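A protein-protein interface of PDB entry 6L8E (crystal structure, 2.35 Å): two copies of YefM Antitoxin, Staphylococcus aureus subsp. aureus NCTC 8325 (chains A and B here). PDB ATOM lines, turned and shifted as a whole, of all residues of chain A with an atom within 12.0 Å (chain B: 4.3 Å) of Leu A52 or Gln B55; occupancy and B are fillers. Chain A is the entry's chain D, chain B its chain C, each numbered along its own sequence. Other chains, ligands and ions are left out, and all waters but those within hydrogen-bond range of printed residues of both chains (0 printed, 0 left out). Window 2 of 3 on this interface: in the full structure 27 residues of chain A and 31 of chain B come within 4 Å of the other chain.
NE2 of Gln B55 is in hydrogen-bond range of O of Leu A52, 3.0 Å away.
Thr A51 touches Leu B52, and with the chains exchanged Leu A52 touches Thr B51. Thr A51 touches Gln B55, but with the chains exchanged Gln A55 does not touch Thr B51 (11.0 Å). Leu A52 touches its own counterpart, Leu B52. Leu A52 touches Gln B55, but with the chains exchanged Gln A55 does not touch Leu B52 (9.1 Å).
Leu A52 touches just these residues of chain B: Thr B51, Leu B52 and Gln B55. Of chain A, only Thr A51 and Leu A52 come within 4 Å of Gln B55. Of the printed residues of chain A, Thr B51 touches Leu A52 (3.6 Å). Leu B52 touches just these residues of chain A: Met A48 (3.7 Å), Thr A51 (3.1 Å) and Leu A52 (3.5 Å). Gln B56 touches none of the printed residues of chain A. Of the printed residues of chain B, Thr A51 touches Leu B52 (3.1 Å) and Gln B55 (3.7 Å). Of the printed residues of chain B, Met A48 touches Leu B52. Printed residues of chain B within 4 Å of Leu A54: Ala B61. Met A49 touches none of the printed residues of chain B. Ser A43 touches none of the printed residues of chain B. The nearest printed residue of chain B that does not touch Leu A52 is Tyr B53 (5.9 Å).
Of the 8 printed residues of chain B, 4 touch a printed residue of chain A. Hydrophobic or aromatic side chains of chain B that line the printed part of chain A: Leu B52 and Ala B61. Among the printed residues, no Asp or Glu carboxylate lies within 4 Å of a Lys or Arg side-chain nitrogen of the other chain.
Met A48 touches Leu B52. Leu B52 touches Thr A51 (CD1 to OG1, 3.1 Å). Thr A51 touches Gln B55. Leu A52 touches Thr B51. CD2 of Leu A52 touches CA of Leu B52, 3.5 Å away. Leu A54 touches Ala B61 (CD1 to CB, 3.7 Å).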
ATOM      1  N   MET A  26      -9.160  -8.049 -22.530  1.00  0.00           N
ATOM      2  CA  MET A  26      -8.457  -7.878 -21.273  1.00  0.00           C
ATOM      3  C   MET A  26      -9.225  -6.944 -20.354  1.00  0.00           C
ATOM      4  O   MET A  26     -10.150  -6.239 -20.767  1.00  0.00           O
ATOM      5  CB  MET A  26      -7.031  -7.345 -21.510  1.00  0.00           C
ATOM      6  CG  MET A  26      -6.251  -8.191 -22.514  1.00  0.00           C
ATOM      7  SD  MET A  26      -4.596  -7.669 -22.979  1.00  0.00           S
ATOM      8  CE  MET A  26      -4.306  -8.729 -24.393  1.00  0.00           C
ATOM      9  N   MET A  40      -5.412 -10.849 -18.512  1.00  0.00           N
ATOM     10  CA  MET A  40      -5.586 -11.411 -19.842  1.00  0.00           C
ATOM     11  C   MET A  40      -5.650 -12.925 -19.726  1.00  0.00           C
ATOM     12  O   MET A  40      -5.233 -13.503 -18.722  1.00  0.00           O
ATOM     13  CB  MET A  40      -4.439 -11.018 -20.780  1.00  0.00           C
ATOM     14  CG  MET A  40      -3.115 -11.677 -20.425  1.00  0.00           C
ATOM     15  SD  MET A  40      -1.697 -10.894 -21.207  1.00  0.00           S
ATOM     16  CE  MET A  40      -1.793  -9.240 -20.533  1.00  0.00           C
ATOM     17  N   SER A  43      -3.941 -18.216 -22.498  1.00  0.00           N
ATOM     18  CA  SER A  43      -3.678 -18.607 -23.879  1.00  0.00           C
ATOM     19  C   SER A  43      -3.251 -17.404 -24.711  1.00  0.00           C
ATOM     20  O   SER A  43      -2.368 -17.513 -25.569  1.00  0.00           O
ATOM     21  CB  SER A  43      -4.914 -19.280 -24.484  1.00  0.00           C
ATOM     22  OG  SER A  43      -6.051 -18.433 -24.417  1.00  0.00           O
ATOM     23  N   ASP A  44      -3.848 -16.237 -24.448  1.00  0.00           N
ATOM     24  CA  ASP A  44      -3.399 -15.024 -25.124  1.00  0.00           C
ATOM     25  C   ASP A  44      -1.987 -14.646 -24.695  1.00  0.00           C
ATOM     26  O   ASP A  44      -1.162 -14.279 -25.535  1.00  0.00           O
ATOM     27  CB  ASP A  44      -4.371 -13.873 -24.865  1.00  0.00           C
ATOM     28  CG  ASP A  44      -5.524 -13.854 -25.846  1.00  0.00           C
ATOM     29  OD1 ASP A  44      -5.464 -14.624 -26.833  1.00  0.00           O
ATOM     30  OD2 ASP A  44      -6.483 -13.079 -25.626  1.00  0.00           O
ATOM     31  N   TYR A  45      -1.688 -14.730 -23.394  1.00  0.00           N
ATOM     32  CA  TYR A  45      -0.333 -14.441 -22.937  1.00  0.00           C
ATOM     33  C   TYR A  45       0.680 -15.323 -23.651  1.00  0.00           C
ATOM     34  O   TYR A  45       1.728 -14.849 -24.106  1.00  0.00           O
ATOM     35  CB  TYR A  45      -0.216 -14.627 -21.428  1.00  0.00           C
ATOM     36  CG  TYR A  45       1.193 -14.400 -20.921  1.00  0.00           C
ATOM     37  CD1 TYR A  45       1.684 -13.111 -20.753  1.00  0.00           C
ATOM     38  CD2 TYR A  45       2.035 -15.465 -20.625  1.00  0.00           C
ATOM     39  CE1 TYR A  45       2.974 -12.888 -20.299  1.00  0.00           C
ATOM     40  CE2 TYR A  45       3.323 -15.255 -20.168  1.00  0.00           C
ATOM     41  CZ  TYR A  45       3.788 -13.969 -20.008  1.00  0.00           C
ATOM     42  OH  TYR A  45       5.073 -13.780 -19.556  1.00  0.00           O
ATOM     43  N   ASN A  46       0.384 -16.620 -23.751  1.00  0.00           N
ATOM     44  CA  ASN A  46       1.331 -17.541 -24.374  1.00  0.00           C
ATOM     45  C   ASN A  46       1.476 -17.258 -25.860  1.00  0.00           C
ATOM     46  O   ASN A  46       2.587 -17.307 -26.398  1.00  0.00           O
ATOM     47  CB  ASN A  46       0.899 -18.988 -24.144  1.00  0.00           C
ATOM     48  CG  ASN A  46       1.042 -19.407 -22.699  1.00  0.00           C
ATOM     49  OD1 ASN A  46       1.923 -18.926 -21.993  1.00  0.00           O
ATOM     50  ND2 ASN A  46       0.171 -20.306 -22.251  1.00  0.00           N
ATOM     51  N   SER A  47       0.361 -16.973 -26.539  1.00  0.00           N
ATOM     52  CA  SER A  47       0.415 -16.623 -27.954  1.00  0.00           C
ATOM     53  C   SER A  47       1.292 -15.397 -28.172  1.00  0.00           C
ATOM     54  O   SER A  47       2.187 -15.405 -29.025  1.00  0.00           O
ATOM     55  CB  SER A  47      -0.996 -16.389 -28.494  1.00  0.00           C
ATOM     56  OG  SER A  47      -1.786 -17.561 -28.381  1.00  0.00           O
ATOM     57  N   MET A  48       1.074 -14.344 -27.375  1.00  0.00           N
ATOM     58  CA  MET A  48       1.825 -13.101 -27.553  1.00  0.00           C
ATOM     59  C   MET A  48       3.308 -13.294 -27.260  1.00  0.00           C
ATOM     60  O   MET A  48       4.159 -12.706 -27.937  1.00  0.00           O
ATOM     61  CB  MET A  48       1.243 -12.000 -26.662  1.00  0.00           C
ATOM     62  CG  MET A  48      -0.210 -11.703 -26.963  1.00  0.00           C
ATOM     63  SD  MET A  48      -0.890 -10.261 -26.132  1.00  0.00           S
ATOM     64  CE  MET A  48      -0.535 -10.664 -24.428  1.00  0.00           C
ATOM     65  N   MET A  49       3.637 -14.107 -26.251  1.00  0.00           N
ATOM     66  CA  MET A  49       5.038 -14.411 -25.968  1.00  0.00           C
ATOM     67  C   MET A  49       5.716 -15.062 -27.167  1.00  0.00           C
ATOM     68  O   MET A  49       6.883 -14.777 -27.464  1.00  0.00           O
ATOM     69  CB  MET A  49       5.136 -15.316 -24.739  1.00  0.00           C
ATOM     70  CG  MET A  49       4.757 -14.618 -23.447  1.00  0.00           C
ATOM     71  SD  MET A  49       5.819 -13.201 -23.133  1.00  0.00           S
ATOM     72  CE  MET A  49       7.406 -14.011 -22.964  1.00  0.00           C
ATOM     73  N   GLU A  50       4.991 -15.930 -27.877  1.00  0.00           N
ATOM     74  CA  GLU A  50       5.570 -16.626 -29.022  1.00  0.00           C
ATOM     75  C   GLU A  50       5.889 -15.659 -30.154  1.00  0.00           C
ATOM     76  O   GLU A  50       6.982 -15.702 -30.732  1.00  0.00           O
ATOM     77  CB  GLU A  50       4.621 -17.724 -29.503  1.00  0.00           C
ATOM     78  CG  GLU A  50       5.164 -18.542 -30.667  1.00  0.00           C
ATOM     79  CD  GLU A  50       4.423 -19.853 -30.865  1.00  0.00           C
ATOM     80  OE1 GLU A  50       3.367 -20.032 -30.225  1.00  0.00           O
ATOM     81  OE2 GLU A  50       4.897 -20.707 -31.647  1.00  0.00           O
ATOM     82  N   THR A  51       4.944 -14.781 -30.498  1.00  0.00           N
ATOM     83  CA  THR A  51       5.207 -13.848 -31.589  1.00  0.00           C
ATOM     84  C   THR A  51       6.236 -12.785 -31.224  1.00  0.00           C
ATOM     85  O   THR A  51       6.708 -12.075 -32.119  1.00  0.00           O
ATOM     86  CB  THR A  51       3.921 -13.156 -32.062  1.00  0.00           C
ATOM     87  OG1 THR A  51       3.877 -11.826 -31.538  1.00  0.00           O
ATOM     88  CG2 THR A  51       2.683 -13.907 -31.610  1.00  0.00           C
ATOM     89  N   LEU A  52       6.584 -12.647 -29.942  1.00  0.00           N
ATOM     90  CA  LEU A  52       7.645 -11.721 -29.558  1.00  0.00           C
ATOM     91  C   LEU A  52       9.013 -12.184 -30.035  1.00  0.00           C
ATOM     92  O   LEU A  52       9.914 -11.355 -30.203  1.00  0.00           O
ATOM     93  CB  LEU A  52       7.676 -11.543 -28.039  1.00  0.00           C
ATOM     94  CG  LEU A  52       6.737 -10.514 -27.420  1.00  0.00           C
ATOM     95  CD1 LEU A  52       7.085 -10.237 -25.959  1.00  0.00           C
ATOM     96  CD2 LEU A  52       6.753  -9.228 -28.223  1.00  0.00           C
ATOM     97  N   TYR A  53       9.191 -13.485 -30.232  1.00  0.00           N
ATOM     98  CA  TYR A  53      10.470 -14.019 -30.668  1.00  0.00           C
ATOM     99  C   TYR A  53      10.623 -13.875 -32.177  1.00  0.00           C
ATOM    100  O   TYR A  53       9.690 -14.134 -32.941  1.00  0.00           O
ATOM    101  CB  TYR A  53      10.592 -15.483 -30.249  1.00  0.00           C
ATOM    102  CG  TYR A  53      11.963 -16.090 -30.440  1.00  0.00           C
ATOM    103  CD1 TYR A  53      12.295 -16.747 -31.621  1.00  0.00           C
ATOM    104  CD2 TYR A  53      12.918 -16.027 -29.434  1.00  0.00           C
ATOM    105  CE1 TYR A  53      13.545 -17.312 -31.798  1.00  0.00           C
ATOM    106  CE2 TYR A  53      14.166 -16.591 -29.601  1.00  0.00           C
ATOM    107  CZ  TYR A  53      14.476 -17.231 -30.782  1.00  0.00           C
ATOM    108  OH  TYR A  53      15.721 -17.792 -30.951  1.00  0.00           O
ATOM    109  N   LEU A  54      11.809 -13.451 -32.599  1.00  0.00           N
ATOM    110  CA  LEU A  54      12.086 -13.219 -34.012  1.00  0.00           C
ATOM    111  C   LEU A  54      12.285 -14.560 -34.706  1.00  0.00           C
ATOM    112  O   LEU A  54      13.340 -15.188 -34.567  1.00  0.00           O
ATOM    113  CB  LEU A  54      13.315 -12.329 -34.171  1.00  0.00           C
ATOM    114  CG  LEU A  54      13.630 -11.796 -35.571  1.00  0.00           C
ATOM    115  CD1 LEU A  54      12.712 -10.637 -35.919  1.00  0.00           C
ATOM    116  CD2 LEU A  54      15.088 -11.379 -35.655  1.00  0.00           C
ATOM    117  N   GLN A  55      11.280 -15.000 -35.457  1.00  0.00           N
ATOM    118  CA  GLN A  55      11.381 -16.244 -36.207  1.00  0.00           C
ATOM    119  C   GLN A  55      11.583 -15.964 -37.690  1.00  0.00           C
ATOM    120  O   GLN A  55      12.704 -15.719 -38.134  1.00  0.00           O
ATOM    121  CB  GLN A  55      10.136 -17.107 -35.997  1.00  0.00           C
ATOM    122  CG  GLN A  55       9.017 -16.404 -35.248  1.00  0.00           C
ATOM    123  CD  GLN A  55       8.793 -16.990 -33.872  1.00  0.00           C
ATOM    124  OE1 GLN A  55       9.368 -18.021 -33.528  1.00  0.00           O
ATOM    125  NE2 GLN A  55       7.957 -16.337 -33.075  1.00  0.00           N
ATOM    126  N   THR B  51       6.385  -3.660 -27.495  1.00  0.00           N
ATOM    127  CA  THR B  51       7.264  -4.592 -28.192  1.00  0.00           C
ATOM    128  C   THR B  51       6.461  -5.517 -29.097  1.00  0.00           C
ATOM    129  O   THR B  51       6.868  -5.787 -30.234  1.00  0.00           O
ATOM    130  CB  THR B  51       8.096  -5.399 -27.196  1.00  0.00           C
ATOM    131  OG1 THR B  51       8.967  -4.517 -26.477  1.00  0.00           O
ATOM    132  CG2 THR B  51       8.949  -6.435 -27.920  1.00  0.00           C
ATOM    133  N   LEU B  52       5.313  -6.003 -28.616  1.00  0.00           N
ATOM    134  CA  LEU B  52       4.451  -6.837 -29.450  1.00  0.00           C
ATOM    135  C   LEU B  52       4.030  -6.099 -30.713  1.00  0.00           C
ATOM    136  O   LEU B  52       3.997  -6.686 -31.802  1.00  0.00           O
ATOM    137  CB  LEU B  52       3.225  -7.289 -28.661  1.00  0.00           C
ATOM    138  CG  LEU B  52       2.233  -8.155 -29.436  1.00  0.00           C
ATOM    139  CD1 LEU B  52       2.875  -9.484 -29.770  1.00  0.00           C
ATOM    140  CD2 LEU B  52       0.953  -8.361 -28.650  1.00  0.00           C
ATOM    141  N   TYR B  53       3.712  -4.808 -30.587  1.00  0.00           N
ATOM    142  CA  TYR B  53       3.286  -4.019 -31.737  1.00  0.00           C
ATOM    143  C   TYR B  53       4.351  -4.019 -32.825  1.00  0.00           C
ATOM    144  O   TYR B  53       4.043  -4.169 -34.014  1.00  0.00           O
ATOM    145  CB  TYR B  53       2.964  -2.590 -31.297  1.00  0.00           C
ATOM    146  CG  TYR B  53       2.585  -1.662 -32.430  1.00  0.00           C
ATOM    147  CD1 TYR B  53       1.409  -1.854 -33.142  1.00  0.00           C
ATOM    148  CD2 TYR B  53       3.396  -0.586 -32.774  1.00  0.00           C
ATOM    149  CE1 TYR B  53       1.052  -1.014 -34.174  1.00  0.00           C
ATOM    150  CE2 TYR B  53       3.045   0.267 -33.807  1.00  0.00           C
ATOM    151  CZ  TYR B  53       1.866   0.044 -34.502  1.00  0.00           C
ATOM    152  OH  TYR B  53       1.481   0.865 -35.537  1.00  0.00           O
ATOM    153  N   LEU B  54       5.619  -3.863 -32.430  1.00  0.00           N
ATOM    154  CA  LEU B  54       6.700  -3.812 -33.405  1.00  0.00           C
ATOM    155  C   LEU B  54       7.053  -5.200 -33.930  1.00  0.00           C
ATOM    156  O   LEU B  54       7.510  -5.327 -35.070  1.00  0.00           O
ATOM    157  CB  LEU B  54       7.930  -3.139 -32.787  1.00  0.00           C
ATOM    158  CG  LEU B  54       7.770  -1.691 -32.320  1.00  0.00           C
ATOM    159  CD1 LEU B  54       8.887  -1.308 -31.361  1.00  0.00           C
ATOM    160  CD2 LEU B  54       7.746  -0.742 -33.506  1.00  0.00           C
ATOM    161  N   GLN B  55       6.833  -6.246 -33.132  1.00  0.00           N
ATOM    162  CA  GLN B  55       7.164  -7.610 -33.537  1.00  0.00           C
ATOM    163  C   GLN B  55       6.030  -8.318 -34.264  1.00  0.00           C
ATOM    164  O   GLN B  55       6.289  -9.277 -34.998  1.00  0.00           O
ATOM    165  CB  GLN B  55       7.557  -8.446 -32.312  1.00  0.00           C
ATOM    166  CG  GLN B  55       8.780  -7.940 -31.565  1.00  0.00           C
ATOM    167  CD  GLN B  55      10.060  -8.108 -32.357  1.00  0.00           C
ATOM    168  OE1 GLN B  55      10.364  -7.316 -33.248  1.00  0.00           O
ATOM    169  NE2 GLN B  55      10.818  -9.153 -32.040  1.00  0.00           N
ATOM    170  N   GLN B  56       4.788  -7.866 -34.072  1.00  0.00           N
ATOM    171  CA  GLN B  56       3.624  -8.570 -34.601  1.00  0.00           C
ATOM    172  C   GLN B  56       3.712  -8.755 -36.109  1.00  0.00           C
ATOM    173  O   GLN B  56       3.437  -9.843 -36.627  1.00  0.00           O
ATOM    174  CB  GLN B  56       2.360  -7.805 -34.237  1.00  0.00           C
ATOM    175  CG  GLN B  56       1.243  -8.635 -33.664  1.00  0.00           C
ATOM    176  CD  GLN B  56       0.223  -7.765 -32.960  1.00  0.00           C
ATOM    177  OE1 GLN B  56       0.327  -6.538 -32.982  1.00  0.00           O
ATOM    178  NE2 GLN B  56      -0.762  -8.391 -32.324  1.00  0.00           N
ATOM    179  N   ASN B  57       4.071  -7.700 -36.825  1.00  0.00           N
ATOM    180  CA  ASN B  57       4.199  -7.759 -38.273  1.00  0.00           C
ATOM    181  C   ASN B  57       5.555  -8.351 -38.635  1.00  0.00           C
ATOM    182  O   ASN B  57       6.586  -7.772 -38.272  1.00  0.00           O
ATOM    183  CB  ASN B  57       4.054  -6.362 -38.870  1.00  0.00           C
ATOM    184  CG  ASN B  57       4.046  -6.363 -40.386  1.00  0.00           C
ATOM    185  OD1 ASN B  57       5.046  -6.690 -41.027  1.00  0.00           O
ATOM    186  ND2 ASN B  57       2.921  -5.969 -40.971  1.00  0.00           N
ATOM    187  N   ALA B  61       9.294  -6.619 -38.018  1.00  0.00           N
ATOM    188  CA  ALA B  61      10.277  -7.280 -37.163  1.00  0.00           C
ATOM    189  C   ALA B  61      11.588  -7.491 -37.912  1.00  0.00           C
ATOM    190  O   ALA B  61      12.671  -7.220 -37.384  1.00  0.00           O
ATOM    191  CB  ALA B  61       9.721  -8.611 -36.647  1.00  0.00           C
